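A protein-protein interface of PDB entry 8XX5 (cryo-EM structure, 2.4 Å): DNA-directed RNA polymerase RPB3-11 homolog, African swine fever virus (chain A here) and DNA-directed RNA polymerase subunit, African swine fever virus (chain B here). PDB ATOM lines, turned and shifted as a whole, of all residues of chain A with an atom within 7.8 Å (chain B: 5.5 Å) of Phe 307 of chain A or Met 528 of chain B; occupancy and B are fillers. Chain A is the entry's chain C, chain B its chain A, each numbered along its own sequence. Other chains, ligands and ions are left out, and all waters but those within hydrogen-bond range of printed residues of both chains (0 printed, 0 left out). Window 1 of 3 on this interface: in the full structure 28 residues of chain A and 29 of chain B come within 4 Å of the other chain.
O of Ser 306 of chain A is in hydrogen-bond range of N of Phe 541 of chain B (2.7 Å).
The backbone NH of Val 308 of chain A is in hydrogen-bond range of the side-chain sulfur of Met 528 of chain B.
The backbone NH (N) of Tyr 310 of chain A lies close to the side-chain amide nitrogen (NE2) of Gln 532 of chain B (3.2 Å).
O of Gln 532 of chain B lies within hydrogen-bond range of NE2 of Gln 311 of chain A (3.4 Å).
The backbone carbonyl oxygen (O) of Ile 305 of chain A lies within hydrogen-bond range of the side-chain amino group (NZ) of Lys 524 of chain B (2.8 Å).
The side-chain amino group of Lys 524 of chain B lies within hydrogen-bond range of the backbone carbonyl oxygen of Pro 303 of chain A (2.8 Å).
O of Ile 324 of chain A sits at hydrogen-bond distance from N of Ser 306 of chain A (3.1 Å).
N of Thr 322 of chain A lies within hydrogen-bond range of O of Gly 309 of chain A, at 2.7 Å.
The side-chain amino group of Lys 524 of chain B lies within hydrogen-bond range of the backbone carbonyl oxygen of Phe 541 of chain B (2.9 Å).
O of Phe 307 of chain A is in hydrogen-bond range of N of Ile 324 of chain A (2.7 Å).
O of Gly 529 of chain B sits close to OE1 of Gln 532 of chain B (3.3 Å).
Lys 524 of chain B touches Tyr 299 of chain A.
Leu 525 of chain B touches Tyr 299 of chain A.
Tyr 299 of chain A touches Met 528 of chain B (CD1 to CE, 3.6 Å).
C of Asp 304 of chain A touches NZ of Lys 524 of chain B (3.6 Å).
O of Ile 305 of chain A touches O of Phe 541 of chain B, at 3.6 Å.
Pro 539 of chain B touches Ser 306 of chain A (O to O, 3.8 Å).
CE1 of Phe 307 of chain A touches O of Met 528 of chain B, at 3.2 Å.
Phe 307 of chain A touches Pro 538 of chain B (CG to CB, 3.4 Å).
NE2 of Gln 532 of chain B touches CA of Gly 309 of chain A, 3.5 Å away.
Ile 324 of chain A touches Pro 538 of chain B.
Phe 307 of chain A touches just these residues of chain B: Met 528 (3.2 Å) and Pro 538 (3.4 Å).
Met 528 of chain B touches just these residues of chain A: Tyr 299 (3.6 Å), Phe 307 (3.2 Å) and Val 308 (3.5 Å).
Of the printed residues of chain B, Gly 309 of chain A touches Gln 532.
Printed residues of chain A within 4 Å of Pro 539 of chain B: Ser 306.
Of the printed residues of chain B, Asp 304 of chain A touches Lys 524.
Of the printed residues of chain A, Phe 541 of chain B touches Ile 305 and Ser 306.
Leu 530 of chain B touches none of the printed residues of chain A.
Ile 298 of chain A touches none of the printed residues of chain B.
The nearest printed residue of chain A that does not touch Pro 538 of chain B is Lys 278 of chain A (4.05 Å).
Hydrophobic or aromatic side chains of chain A that line the printed part of chain B: Tyr 299, Phe 307, Val 308, Tyr 310 and Ile 324.
Of the 13 printed residues of chain B, 7 touch a printed residue of chain A.
Along chain B the printed residues that touch a printed residue of chain A span positions 524 to 541.
Among the printed residues, no Asp or Glu carboxylate lies within 4 Å of a Lys or Arg side-chain nitrogen of the other chain.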
ATOM      1  N   LYS A 276      -9.669 -17.439  21.834  1.00  0.00           N
ATOM      2  CA  LYS A 276      -8.765 -16.841  20.865  1.00  0.00           C
ATOM      3  C   LYS A 276      -8.670 -17.701  19.615  1.00  0.00           C
ATOM      4  O   LYS A 276      -8.750 -18.930  19.681  1.00  0.00           O
ATOM      5  CB  LYS A 276      -7.374 -16.673  21.476  1.00  0.00           C
ATOM      6  CG  LYS A 276      -7.052 -15.267  21.936  1.00  0.00           C
ATOM      7  CD  LYS A 276      -5.702 -15.228  22.632  1.00  0.00           C
ATOM      8  CE  LYS A 276      -5.630 -14.100  23.640  1.00  0.00           C
ATOM      9  NZ  LYS A 276      -4.902 -14.510  24.871  1.00  0.00           N
ATOM     10  N   THR A 277      -8.500 -17.046  18.473  1.00  0.00           N
ATOM     11  CA  THR A 277      -8.236 -17.724  17.213  1.00  0.00           C
ATOM     12  C   THR A 277      -6.911 -17.226  16.657  1.00  0.00           C
ATOM     13  O   THR A 277      -6.662 -16.018  16.620  1.00  0.00           O
ATOM     14  CB  THR A 277      -9.366 -17.495  16.200  1.00  0.00           C
ATOM     15  OG1 THR A 277      -8.945 -17.938  14.904  1.00  0.00           O
ATOM     16  CG2 THR A 277      -9.744 -16.025  16.130  1.00  0.00           C
ATOM     17  N   LYS A 278      -6.059 -18.157  16.242  1.00  0.00           N
ATOM     18  CA  LYS A 278      -4.778 -17.827  15.640  1.00  0.00           C
ATOM     19  C   LYS A 278      -4.846 -18.074  14.141  1.00  0.00           C
ATOM     20  O   LYS A 278      -5.221 -19.165  13.703  1.00  0.00           O
ATOM     21  CB  LYS A 278      -3.645 -18.648  16.257  1.00  0.00           C
ATOM     22  CG  LYS A 278      -2.284 -18.347  15.655  1.00  0.00           C
ATOM     23  CD  LYS A 278      -1.296 -19.466  15.916  1.00  0.00           C
ATOM     24  CE  LYS A 278      -0.792 -19.435  17.346  1.00  0.00           C
ATOM     25  NZ  LYS A 278       0.643 -19.048  17.413  1.00  0.00           N
ATOM     26  N   ALA A 279      -4.490 -17.057  13.362  1.00  0.00           N
ATOM     27  CA  ALA A 279      -4.439 -17.151  11.910  1.00  0.00           C
ATOM     28  C   ALA A 279      -2.995 -16.983  11.468  1.00  0.00           C
ATOM     29  O   ALA A 279      -2.339 -16.006  11.841  1.00  0.00           O
ATOM     30  CB  ALA A 279      -5.331 -16.094  11.257  1.00  0.00           C
ATOM     31  N   LYS A 295       0.612  -6.071   8.645  1.00  0.00           N
ATOM     32  CA  LYS A 295       0.670  -5.917  10.093  1.00  0.00           C
ATOM     33  C   LYS A 295       0.192  -4.535  10.515  1.00  0.00           C
ATOM     34  O   LYS A 295      -0.585  -4.406  11.467  1.00  0.00           O
ATOM     35  CB  LYS A 295       2.088  -6.175  10.599  1.00  0.00           C
ATOM     36  CG  LYS A 295       2.268  -5.883  12.078  1.00  0.00           C
ATOM     37  CD  LYS A 295       3.649  -6.274  12.564  1.00  0.00           C
ATOM     38  CE  LYS A 295       4.706  -5.294  12.084  1.00  0.00           C
ATOM     39  NZ  LYS A 295       4.157  -3.924  11.904  1.00  0.00           N
ATOM     40  N   ILE A 298      -3.703  -4.294   9.933  1.00  0.00           N
ATOM     41  CA  ILE A 298      -4.417  -5.163  10.863  1.00  0.00           C
ATOM     42  C   ILE A 298      -4.377  -4.575  12.266  1.00  0.00           C
ATOM     43  O   ILE A 298      -5.387  -4.557  12.978  1.00  0.00           O
ATOM     44  CB  ILE A 298      -3.826  -6.585  10.826  1.00  0.00           C
ATOM     45  CG1 ILE A 298      -4.209  -7.291   9.527  1.00  0.00           C
ATOM     46  CG2 ILE A 298      -4.297  -7.394  12.019  1.00  0.00           C
ATOM     47  CD1 ILE A 298      -3.321  -8.462   9.184  1.00  0.00           C
ATOM     48  N   TYR A 299      -3.211  -4.075  12.679  1.00  0.00           N
ATOM     49  CA  TYR A 299      -3.078  -3.462  13.992  1.00  0.00           C
ATOM     50  C   TYR A 299      -3.893  -2.180  14.098  1.00  0.00           C
ATOM     51  O   TYR A 299      -4.445  -1.885  15.163  1.00  0.00           O
ATOM     52  CB  TYR A 299      -1.598  -3.206  14.266  1.00  0.00           C
ATOM     53  CG  TYR A 299      -1.288  -2.413  15.506  1.00  0.00           C
ATOM     54  CD1 TYR A 299      -1.418  -2.979  16.766  1.00  0.00           C
ATOM     55  CD2 TYR A 299      -0.823  -1.111  15.417  1.00  0.00           C
ATOM     56  CE1 TYR A 299      -1.115  -2.262  17.900  1.00  0.00           C
ATOM     57  CE2 TYR A 299      -0.520  -0.388  16.543  1.00  0.00           C
ATOM     58  CZ  TYR A 299      -0.667  -0.967  17.781  1.00  0.00           C
ATOM     59  OH  TYR A 299      -0.358  -0.244  18.905  1.00  0.00           O
ATOM     60  N   ILE A 302      -7.502  -3.481  14.357  1.00  0.00           N
ATOM     61  CA  ILE A 302      -7.726  -4.171  15.625  1.00  0.00           C
ATOM     62  C   ILE A 302      -6.717  -3.656  16.642  1.00  0.00           C
ATOM     63  O   ILE A 302      -5.706  -4.325  16.901  1.00  0.00           O
ATOM     64  CB  ILE A 302      -7.614  -5.696  15.471  1.00  0.00           C
ATOM     65  CG1 ILE A 302      -8.250  -6.159  14.160  1.00  0.00           C
ATOM     66  CG2 ILE A 302      -8.263  -6.396  16.650  1.00  0.00           C
ATOM     67  CD1 ILE A 302      -8.057  -7.627  13.881  1.00  0.00           C
ATOM     68  N   PRO A 303      -6.936  -2.477  17.228  1.00  0.00           N
ATOM     69  CA  PRO A 303      -5.999  -1.985  18.250  1.00  0.00           C
ATOM     70  C   PRO A 303      -5.911  -2.884  19.468  1.00  0.00           C
ATOM     71  O   PRO A 303      -4.879  -2.893  20.148  1.00  0.00           O
ATOM     72  CB  PRO A 303      -6.567  -0.605  18.605  1.00  0.00           C
ATOM     73  CG  PRO A 303      -8.005  -0.681  18.234  1.00  0.00           C
ATOM     74  CD  PRO A 303      -8.063  -1.554  17.021  1.00  0.00           C
ATOM     75  N   ASP A 304      -6.965  -3.643  19.761  1.00  0.00           N
ATOM     76  CA  ASP A 304      -7.003  -4.551  20.897  1.00  0.00           C
ATOM     77  C   ASP A 304      -6.524  -5.953  20.543  1.00  0.00           C
ATOM     78  O   ASP A 304      -6.894  -6.915  21.225  1.00  0.00           O
ATOM     79  CB  ASP A 304      -8.420  -4.616  21.467  1.00  0.00           C
ATOM     80  CG  ASP A 304      -9.460  -4.917  20.403  1.00  0.00           C
ATOM     81  OD1 ASP A 304      -9.547  -4.149  19.422  1.00  0.00           O
ATOM     82  OD2 ASP A 304     -10.189  -5.919  20.547  1.00  0.00           O
ATOM     83  N   ILE A 305      -5.715  -6.089  19.489  1.00  0.00           N
ATOM     84  CA  ILE A 305      -5.274  -7.405  19.051  1.00  0.00           C
ATOM     85  C   ILE A 305      -4.403  -8.044  20.124  1.00  0.00           C
ATOM     86  O   ILE A 305      -3.655  -7.365  20.837  1.00  0.00           O
ATOM     87  CB  ILE A 305      -4.531  -7.295  17.709  1.00  0.00           C
ATOM     88  CG1 ILE A 305      -4.338  -8.677  17.083  1.00  0.00           C
ATOM     89  CG2 ILE A 305      -3.197  -6.581  17.879  1.00  0.00           C
ATOM     90  CD1 ILE A 305      -5.427  -9.058  16.118  1.00  0.00           C
ATOM     91  N   SER A 306      -4.525  -9.364  20.266  1.00  0.00           N
ATOM     92  CA  SER A 306      -3.664 -10.085  21.196  1.00  0.00           C
ATOM     93  C   SER A 306      -2.227 -10.117  20.691  1.00  0.00           C
ATOM     94  O   SER A 306      -1.286  -9.855  21.446  1.00  0.00           O
ATOM     95  CB  SER A 306      -4.196 -11.499  21.416  1.00  0.00           C
ATOM     96  OG  SER A 306      -3.251 -12.294  22.109  1.00  0.00           O
ATOM     97  N   PHE A 307      -2.042 -10.434  19.411  1.00  0.00           N
ATOM     98  CA  PHE A 307      -0.720 -10.404  18.800  1.00  0.00           C
ATOM     99  C   PHE A 307      -0.871 -10.367  17.290  1.00  0.00           C
ATOM    100  O   PHE A 307      -1.679 -11.113  16.729  1.00  0.00           O
ATOM    101  CB  PHE A 307       0.118 -11.618  19.213  1.00  0.00           C
ATOM    102  CG  PHE A 307       1.492 -11.637  18.605  1.00  0.00           C
ATOM    103  CD1 PHE A 307       2.526 -10.921  19.180  1.00  0.00           C
ATOM    104  CD2 PHE A 307       1.745 -12.364  17.453  1.00  0.00           C
ATOM    105  CE1 PHE A 307       3.788 -10.935  18.623  1.00  0.00           C
ATOM    106  CE2 PHE A 307       3.005 -12.380  16.894  1.00  0.00           C
ATOM    107  CZ  PHE A 307       4.026 -11.664  17.479  1.00  0.00           C
ATOM    108  N   VAL A 308      -0.098  -9.505  16.642  1.00  0.00           N
ATOM    109  CA  VAL A 308       0.051  -9.514  15.192  1.00  0.00           C
ATOM    110  C   VAL A 308       1.525  -9.302  14.875  1.00  0.00           C
ATOM    111  O   VAL A 308       2.205  -8.508  15.532  1.00  0.00           O
ATOM    112  CB  VAL A 308      -0.840  -8.454  14.507  1.00  0.00           C
ATOM    113  CG1 VAL A 308      -0.467  -7.053  14.949  1.00  0.00           C
ATOM    114  CG2 VAL A 308      -0.763  -8.586  12.995  1.00  0.00           C
ATOM    115  N   GLY A 309       2.025 -10.039  13.893  1.00  0.00           N
ATOM    116  CA  GLY A 309       3.421  -9.925  13.518  1.00  0.00           C
ATOM    117  C   GLY A 309       3.711 -10.776  12.304  1.00  0.00           C
ATOM    118  O   GLY A 309       2.893 -11.596  11.880  1.00  0.00           O
ATOM    119  N   TYR A 310       4.900 -10.568  11.751  1.00  0.00           N
ATOM    120  CA  TYR A 310       5.335 -11.295  10.570  1.00  0.00           C
ATOM    121  C   TYR A 310       6.835 -11.528  10.649  1.00  0.00           C
ATOM    122  O   TYR A 310       7.555 -10.840  11.375  1.00  0.00           O
ATOM    123  CB  TYR A 310       4.977 -10.545   9.282  1.00  0.00           C
ATOM    124  CG  TYR A 310       5.905  -9.399   8.956  1.00  0.00           C
ATOM    125  CD1 TYR A 310       5.804  -8.188   9.623  1.00  0.00           C
ATOM    126  CD2 TYR A 310       6.879  -9.527   7.978  1.00  0.00           C
ATOM    127  CE1 TYR A 310       6.648  -7.140   9.328  1.00  0.00           C
ATOM    128  CE2 TYR A 310       7.727  -8.486   7.676  1.00  0.00           C
ATOM    129  CZ  TYR A 310       7.608  -7.294   8.353  1.00  0.00           C
ATOM    130  OH  TYR A 310       8.454  -6.254   8.051  1.00  0.00           O
ATOM    131  N   GLN A 311       7.300 -12.518   9.891  1.00  0.00           N
ATOM    132  CA  GLN A 311       8.724 -12.809   9.791  1.00  0.00           C
ATOM    133  C   GLN A 311       9.056 -13.137   8.345  1.00  0.00           C
ATOM    134  O   GLN A 311       8.551 -14.122   7.799  1.00  0.00           O
ATOM    135  CB  GLN A 311       9.123 -13.966  10.713  1.00  0.00           C
ATOM    136  CG  GLN A 311       8.107 -15.090  10.782  1.00  0.00           C
ATOM    137  CD  GLN A 311       8.312 -15.981  11.988  1.00  0.00           C
ATOM    138  OE1 GLN A 311       7.368 -16.596  12.488  1.00  0.00           O
ATOM    139  NE2 GLN A 311       9.549 -16.057  12.465  1.00  0.00           N
ATOM    140  N   LEU A 321       2.780 -14.347   8.338  1.00  0.00           N
ATOM    141  CA  LEU A 321       2.064 -13.374   9.149  1.00  0.00           C
ATOM    142  C   LEU A 321       1.171 -14.105  10.143  1.00  0.00           C
ATOM    143  O   LEU A 321       0.347 -14.934   9.749  1.00  0.00           O
ATOM    144  CB  LEU A 321       1.231 -12.441   8.270  1.00  0.00           C
ATOM    145  CG  LEU A 321       0.307 -11.452   8.979  1.00  0.00           C
ATOM    146  CD1 LEU A 321       1.086 -10.255   9.488  1.00  0.00           C
ATOM    147  CD2 LEU A 321      -0.800 -11.009   8.043  1.00  0.00           C
ATOM    148  N   THR A 322       1.339 -13.794  11.424  1.00  0.00           N
ATOM    149  CA  THR A 322       0.613 -14.451  12.502  1.00  0.00           C
ATOM    150  C   THR A 322      -0.305 -13.447  13.185  1.00  0.00           C
ATOM    151  O   THR A 322       0.149 -12.390  13.633  1.00  0.00           O
ATOM    152  CB  THR A 322       1.579 -15.056  13.521  1.00  0.00           C
ATOM    153  OG1 THR A 322       2.344 -16.095  12.899  1.00  0.00           O
ATOM    154  CG2 THR A 322       0.818 -15.635  14.701  1.00  0.00           C
ATOM    155  N   ILE A 323      -1.590 -13.780  13.262  1.00  0.00           N
ATOM    156  CA  ILE A 323      -2.590 -12.947  13.918  1.00  0.00           C
ATOM    157  C   ILE A 323      -3.263 -13.774  15.003  1.00  0.00           C
ATOM    158  O   ILE A 323      -3.760 -14.872  14.733  1.00  0.00           O
ATOM    159  CB  ILE A 323      -3.632 -12.413  12.920  1.00  0.00           C
ATOM    160  CG1 ILE A 323      -2.953 -11.623  11.803  1.00  0.00           C
ATOM    161  CG2 ILE A 323      -4.651 -11.547  13.632  1.00  0.00           C
ATOM    162  CD1 ILE A 323      -3.467 -11.965  10.431  1.00  0.00           C
ATOM    163  N   ILE A 324      -3.275 -13.248  16.223  1.00  0.00           N
ATOM    164  CA  ILE A 324      -3.966 -13.864  17.348  1.00  0.00           C
ATOM    165  C   ILE A 324      -4.952 -12.849  17.902  1.00  0.00           C
ATOM    166  O   ILE A 324      -4.569 -11.716  18.215  1.00  0.00           O
ATOM    167  CB  ILE A 324      -2.983 -14.328  18.437  1.00  0.00           C
ATOM    168  CG1 ILE A 324      -1.910 -15.233  17.831  1.00  0.00           C
ATOM    169  CG2 ILE A 324      -3.728 -15.039  19.550  1.00  0.00           C
ATOM    170  CD1 ILE A 324      -1.165 -16.066  18.842  1.00  0.00           C
ATOM    171  N   HIS A 325      -6.215 -13.248  18.019  1.00  0.00           N
ATOM    172  CA  HIS A 325      -7.255 -12.322  18.441  1.00  0.00           C
ATOM    173  C   HIS A 325      -8.312 -13.059  19.247  1.00  0.00           C
ATOM    174  O   HIS A 325      -8.642 -14.208  18.948  1.00  0.00           O
ATOM    175  CB  HIS A 325      -7.900 -11.632  17.235  1.00  0.00           C
ATOM    176  CG  HIS A 325      -8.800 -10.495  17.602  1.00  0.00           C
ATOM    177  ND1 HIS A 325      -8.648  -9.773  18.765  1.00  0.00           N
ATOM    178  CD2 HIS A 325      -9.863  -9.958  16.961  1.00  0.00           C
ATOM    179  CE1 HIS A 325      -9.577  -8.837  18.824  1.00  0.00           C
ATOM    180  NE2 HIS A 325     -10.328  -8.928  17.741  1.00  0.00           N
ATOM    181  N   LYS A 326      -8.843 -12.381  20.266  1.00  0.00           N
ATOM    182  CA  LYS A 326      -9.958 -12.896  21.063  1.00  0.00           C
ATOM    183  C   LYS A 326     -11.240 -12.720  20.256  1.00  0.00           C
ATOM    184  O   LYS A 326     -12.066 -11.841  20.511  1.00  0.00           O
ATOM    185  CB  LYS A 326     -10.043 -12.178  22.403  1.00  0.00           C
ATOM    186  CG  LYS A 326      -9.219 -12.797  23.512  1.00  0.00           C
ATOM    187  CD  LYS A 326      -8.501 -11.724  24.312  1.00  0.00           C
ATOM    188  CE  LYS A 326      -8.467 -12.062  25.792  1.00  0.00           C
ATOM    189  NZ  LYS A 326      -7.587 -13.224  26.085  1.00  0.00           N
ATOM    190  N   LEU A 332     -12.653 -12.741  12.664  1.00  0.00           N
ATOM    191  CA  LEU A 332     -11.268 -12.445  12.323  1.00  0.00           C
ATOM    192  C   LEU A 332     -11.100 -12.272  10.821  1.00  0.00           C
ATOM    193  O   LEU A 332     -10.401 -11.358  10.371  1.00  0.00           O
ATOM    194  CB  LEU A 332     -10.350 -13.552  12.840  1.00  0.00           C
ATOM    195  CG  LEU A 332      -8.850 -13.279  12.713  1.00  0.00           C
ATOM    196  CD1 LEU A 332      -8.500 -11.930  13.317  1.00  0.00           C
ATOM    197  CD2 LEU A 332      -8.039 -14.390  13.360  1.00  0.00           C
ATOM    198  N   ASN B 523       5.878   1.260  22.430  1.00  0.00           N
ATOM    199  CA  ASN B 523       4.437   1.107  22.341  1.00  0.00           C
ATOM    200  C   ASN B 523       4.087  -0.364  22.124  1.00  0.00           C
ATOM    201  O   ASN B 523       4.956  -1.236  22.056  1.00  0.00           O
ATOM    202  CB  ASN B 523       3.867   1.999  21.239  1.00  0.00           C
ATOM    203  CG  ASN B 523       4.539   1.789  19.898  1.00  0.00           C
ATOM    204  OD1 ASN B 523       5.208   0.783  19.671  1.00  0.00           O
ATOM    205  ND2 ASN B 523       4.357   2.741  18.994  1.00  0.00           N
ATOM    206  N   LYS B 524       2.787  -0.646  22.023  1.00  0.00           N
ATOM    207  CA  LYS B 524       2.338  -2.027  21.881  1.00  0.00           C
ATOM    208  C   LYS B 524       2.809  -2.634  20.564  1.00  0.00           C
ATOM    209  O   LYS B 524       3.170  -3.815  20.515  1.00  0.00           O
ATOM    210  CB  LYS B 524       0.815  -2.090  21.993  1.00  0.00           C
ATOM    211  CG  LYS B 524       0.205  -3.407  21.560  1.00  0.00           C
ATOM    212  CD  LYS B 524      -1.303  -3.306  21.481  1.00  0.00           C
ATOM    213  CE  LYS B 524      -1.930  -4.660  21.224  1.00  0.00           C
ATOM    214  NZ  LYS B 524      -3.342  -4.706  21.680  1.00  0.00           N
ATOM    215  N   LEU B 525       2.813  -1.843  19.489  1.00  0.00           N
ATOM    216  CA  LEU B 525       3.208  -2.367  18.187  1.00  0.00           C
ATOM    217  C   LEU B 525       4.660  -2.829  18.188  1.00  0.00           C
ATOM    218  O   LEU B 525       4.981  -3.895  17.650  1.00  0.00           O
ATOM    219  CB  LEU B 525       2.987  -1.310  17.107  1.00  0.00           C
ATOM    220  CG  LEU B 525       3.169  -1.787  15.666  1.00  0.00           C
ATOM    221  CD1 LEU B 525       2.357  -3.047  15.414  1.00  0.00           C
ATOM    222  CD2 LEU B 525       2.787  -0.695  14.685  1.00  0.00           C
ATOM    223  N   HIS B 526       5.554  -2.039  18.782  1.00  0.00           N
ATOM    224  CA  HIS B 526       6.961  -2.416  18.820  1.00  0.00           C
ATOM    225  C   HIS B 526       7.243  -3.482  19.868  1.00  0.00           C
ATOM    226  O   HIS B 526       8.185  -4.265  19.705  1.00  0.00           O
ATOM    227  CB  HIS B 526       7.826  -1.181  19.061  1.00  0.00           C
ATOM    228  CG  HIS B 526       7.868  -0.248  17.892  1.00  0.00           C
ATOM    229  ND1 HIS B 526       6.923   0.734  17.689  1.00  0.00           N
ATOM    230  CD2 HIS B 526       8.732  -0.159  16.854  1.00  0.00           C
ATOM    231  CE1 HIS B 526       7.207   1.393  16.581  1.00  0.00           C
ATOM    232  NE2 HIS B 526       8.300   0.871  16.055  1.00  0.00           N
ATOM    233  N   ALA B 527       6.456  -3.526  20.944  1.00  0.00           N
ATOM    234  CA  ALA B 527       6.575  -4.625  21.893  1.00  0.00           C
ATOM    235  C   ALA B 527       6.193  -5.948  21.246  1.00  0.00           C
ATOM    236  O   ALA B 527       6.838  -6.976  21.483  1.00  0.00           O
ATOM    237  CB  ALA B 527       5.711  -4.354  23.124  1.00  0.00           C
ATOM    238  N   MET B 528       5.140  -5.943  20.425  1.00  0.00           N
ATOM    239  CA  MET B 528       4.770  -7.141  19.681  1.00  0.00           C
ATOM    240  C   MET B 528       5.850  -7.522  18.677  1.00  0.00           C
ATOM    241  O   MET B 528       6.138  -8.709  18.484  1.00  0.00           O
ATOM    242  CB  MET B 528       3.434  -6.926  18.972  1.00  0.00           C
ATOM    243  CG  MET B 528       2.232  -6.935  19.893  1.00  0.00           C
ATOM    244  SD  MET B 528       0.677  -7.026  18.994  1.00  0.00           S
ATOM    245  CE  MET B 528       0.809  -5.571  17.962  1.00  0.00           C
ATOM    246  N   GLY B 529       6.457  -6.529  18.024  1.00  0.00           N
ATOM    247  CA  GLY B 529       7.490  -6.801  17.042  1.00  0.00           C
ATOM    248  C   GLY B 529       8.739  -7.429  17.620  1.00  0.00           C
ATOM    249  O   GLY B 529       9.528  -8.019  16.875  1.00  0.00           O
ATOM    250  N   LEU B 530       8.942  -7.313  18.932  1.00  0.00           N
ATOM    251  CA  LEU B 530      10.085  -7.957  19.565  1.00  0.00           C
ATOM    252  C   LEU B 530       9.947  -9.474  19.563  1.00  0.00           C
ATOM    253  O   LEU B 530      10.957 -10.187  19.574  1.00  0.00           O
ATOM    254  CB  LEU B 530      10.249  -7.439  20.992  1.00  0.00           C
ATOM    255  CG  LEU B 530      11.384  -6.445  21.240  1.00  0.00           C
ATOM    256  CD1 LEU B 530      11.355  -5.326  20.220  1.00  0.00           C
ATOM    257  CD2 LEU B 530      11.292  -5.887  22.645  1.00  0.00           C
ATOM    258  N   PHE B 531       8.717  -9.981  19.544  1.00  0.00           N
ATOM    259  CA  PHE B 531       8.449 -11.411  19.601  1.00  0.00           C
ATOM    260  C   PHE B 531       8.169 -12.012  18.232  1.00  0.00           C
ATOM    261  O   PHE B 531       7.728 -13.162  18.151  1.00  0.00           O
ATOM    262  CB  PHE B 531       7.275 -11.687  20.540  1.00  0.00           C
ATOM    263  CG  PHE B 531       7.562 -11.383  21.980  1.00  0.00           C
ATOM    264  CD1 PHE B 531       7.358 -10.113  22.487  1.00  0.00           C
ATOM    265  CD2 PHE B 531       8.035 -12.368  22.828  1.00  0.00           C
ATOM    266  CE1 PHE B 531       7.620  -9.830  23.811  1.00  0.00           C
ATOM    267  CE2 PHE B 531       8.299 -12.090  24.153  1.00  0.00           C
ATOM    268  CZ  PHE B 531       8.092 -10.820  24.645  1.00  0.00           C
ATOM    269  N   GLN B 532       8.407 -11.261  17.156  1.00  0.00           N
ATOM    270  CA  GLN B 532       8.101 -11.759  15.820  1.00  0.00           C
ATOM    271  C   GLN B 532       8.959 -12.965  15.456  1.00  0.00           C
ATOM    272  O   GLN B 532       8.465 -13.926  14.856  1.00  0.00           O
ATOM    273  CB  GLN B 532       8.292 -10.646  14.791  1.00  0.00           C
ATOM    274  CG  GLN B 532       7.110  -9.717  14.658  1.00  0.00           C
ATOM    275  CD  GLN B 532       7.412  -8.539  13.763  1.00  0.00           C
ATOM    276  OE1 GLN B 532       8.534  -8.040  13.736  1.00  0.00           O
ATOM    277  NE2 GLN B 532       6.410  -8.085  13.024  1.00  0.00           N
ATOM    278  N   PRO B 538       3.571 -16.387  20.928  1.00  0.00           N
ATOM    279  CA  PRO B 538       3.700 -15.005  21.377  1.00  0.00           C
ATOM    280  C   PRO B 538       2.898 -14.763  22.640  1.00  0.00           C
ATOM    281  O   PRO B 538       1.869 -15.420  22.878  1.00  0.00           O
ATOM    282  CB  PRO B 538       3.142 -14.195  20.194  1.00  0.00           C
ATOM    283  CG  PRO B 538       2.276 -15.143  19.457  1.00  0.00           C
ATOM    284  CD  PRO B 538       2.867 -16.500  19.640  1.00  0.00           C
ATOM    285  N   PRO B 539       3.332 -13.836  23.490  1.00  0.00           N
ATOM    286  CA  PRO B 539       2.522 -13.454  24.649  1.00  0.00           C
ATOM    287  C   PRO B 539       1.306 -12.649  24.219  1.00  0.00           C
ATOM    288  O   PRO B 539       1.204 -12.159  23.093  1.00  0.00           O
ATOM    289  CB  PRO B 539       3.480 -12.618  25.500  1.00  0.00           C
ATOM    290  CG  PRO B 539       4.504 -12.123  24.547  1.00  0.00           C
ATOM    291  CD  PRO B 539       4.636 -13.153  23.468  1.00  0.00           C
ATOM    292  N   PHE B 541      -0.977  -9.509  24.144  1.00  0.00           N
ATOM    293  CA  PHE B 541      -0.949  -8.059  24.272  1.00  0.00           C
ATOM    294  C   PHE B 541      -2.343  -7.450  24.214  1.00  0.00           C
ATOM    295  O   PHE B 541      -2.470  -6.236  24.031  1.00  0.00           O
ATOM    296  CB  PHE B 541      -0.067  -7.445  23.184  1.00  0.00           C
ATOM    297  CG  PHE B 541       1.388  -7.787  23.313  1.00  0.00           C
ATOM    298  CD1 PHE B 541       1.888  -8.962  22.778  1.00  0.00           C
ATOM    299  CD2 PHE B 541       2.260  -6.931  23.963  1.00  0.00           C
ATOM    300  CE1 PHE B 541       3.224  -9.277  22.893  1.00  0.00           C
ATOM    301  CE2 PHE B 541       3.597  -7.243  24.082  1.00  0.00           C
ATOM    302  CZ  PHE B 541       4.079  -8.418  23.546  1.00  0.00           C
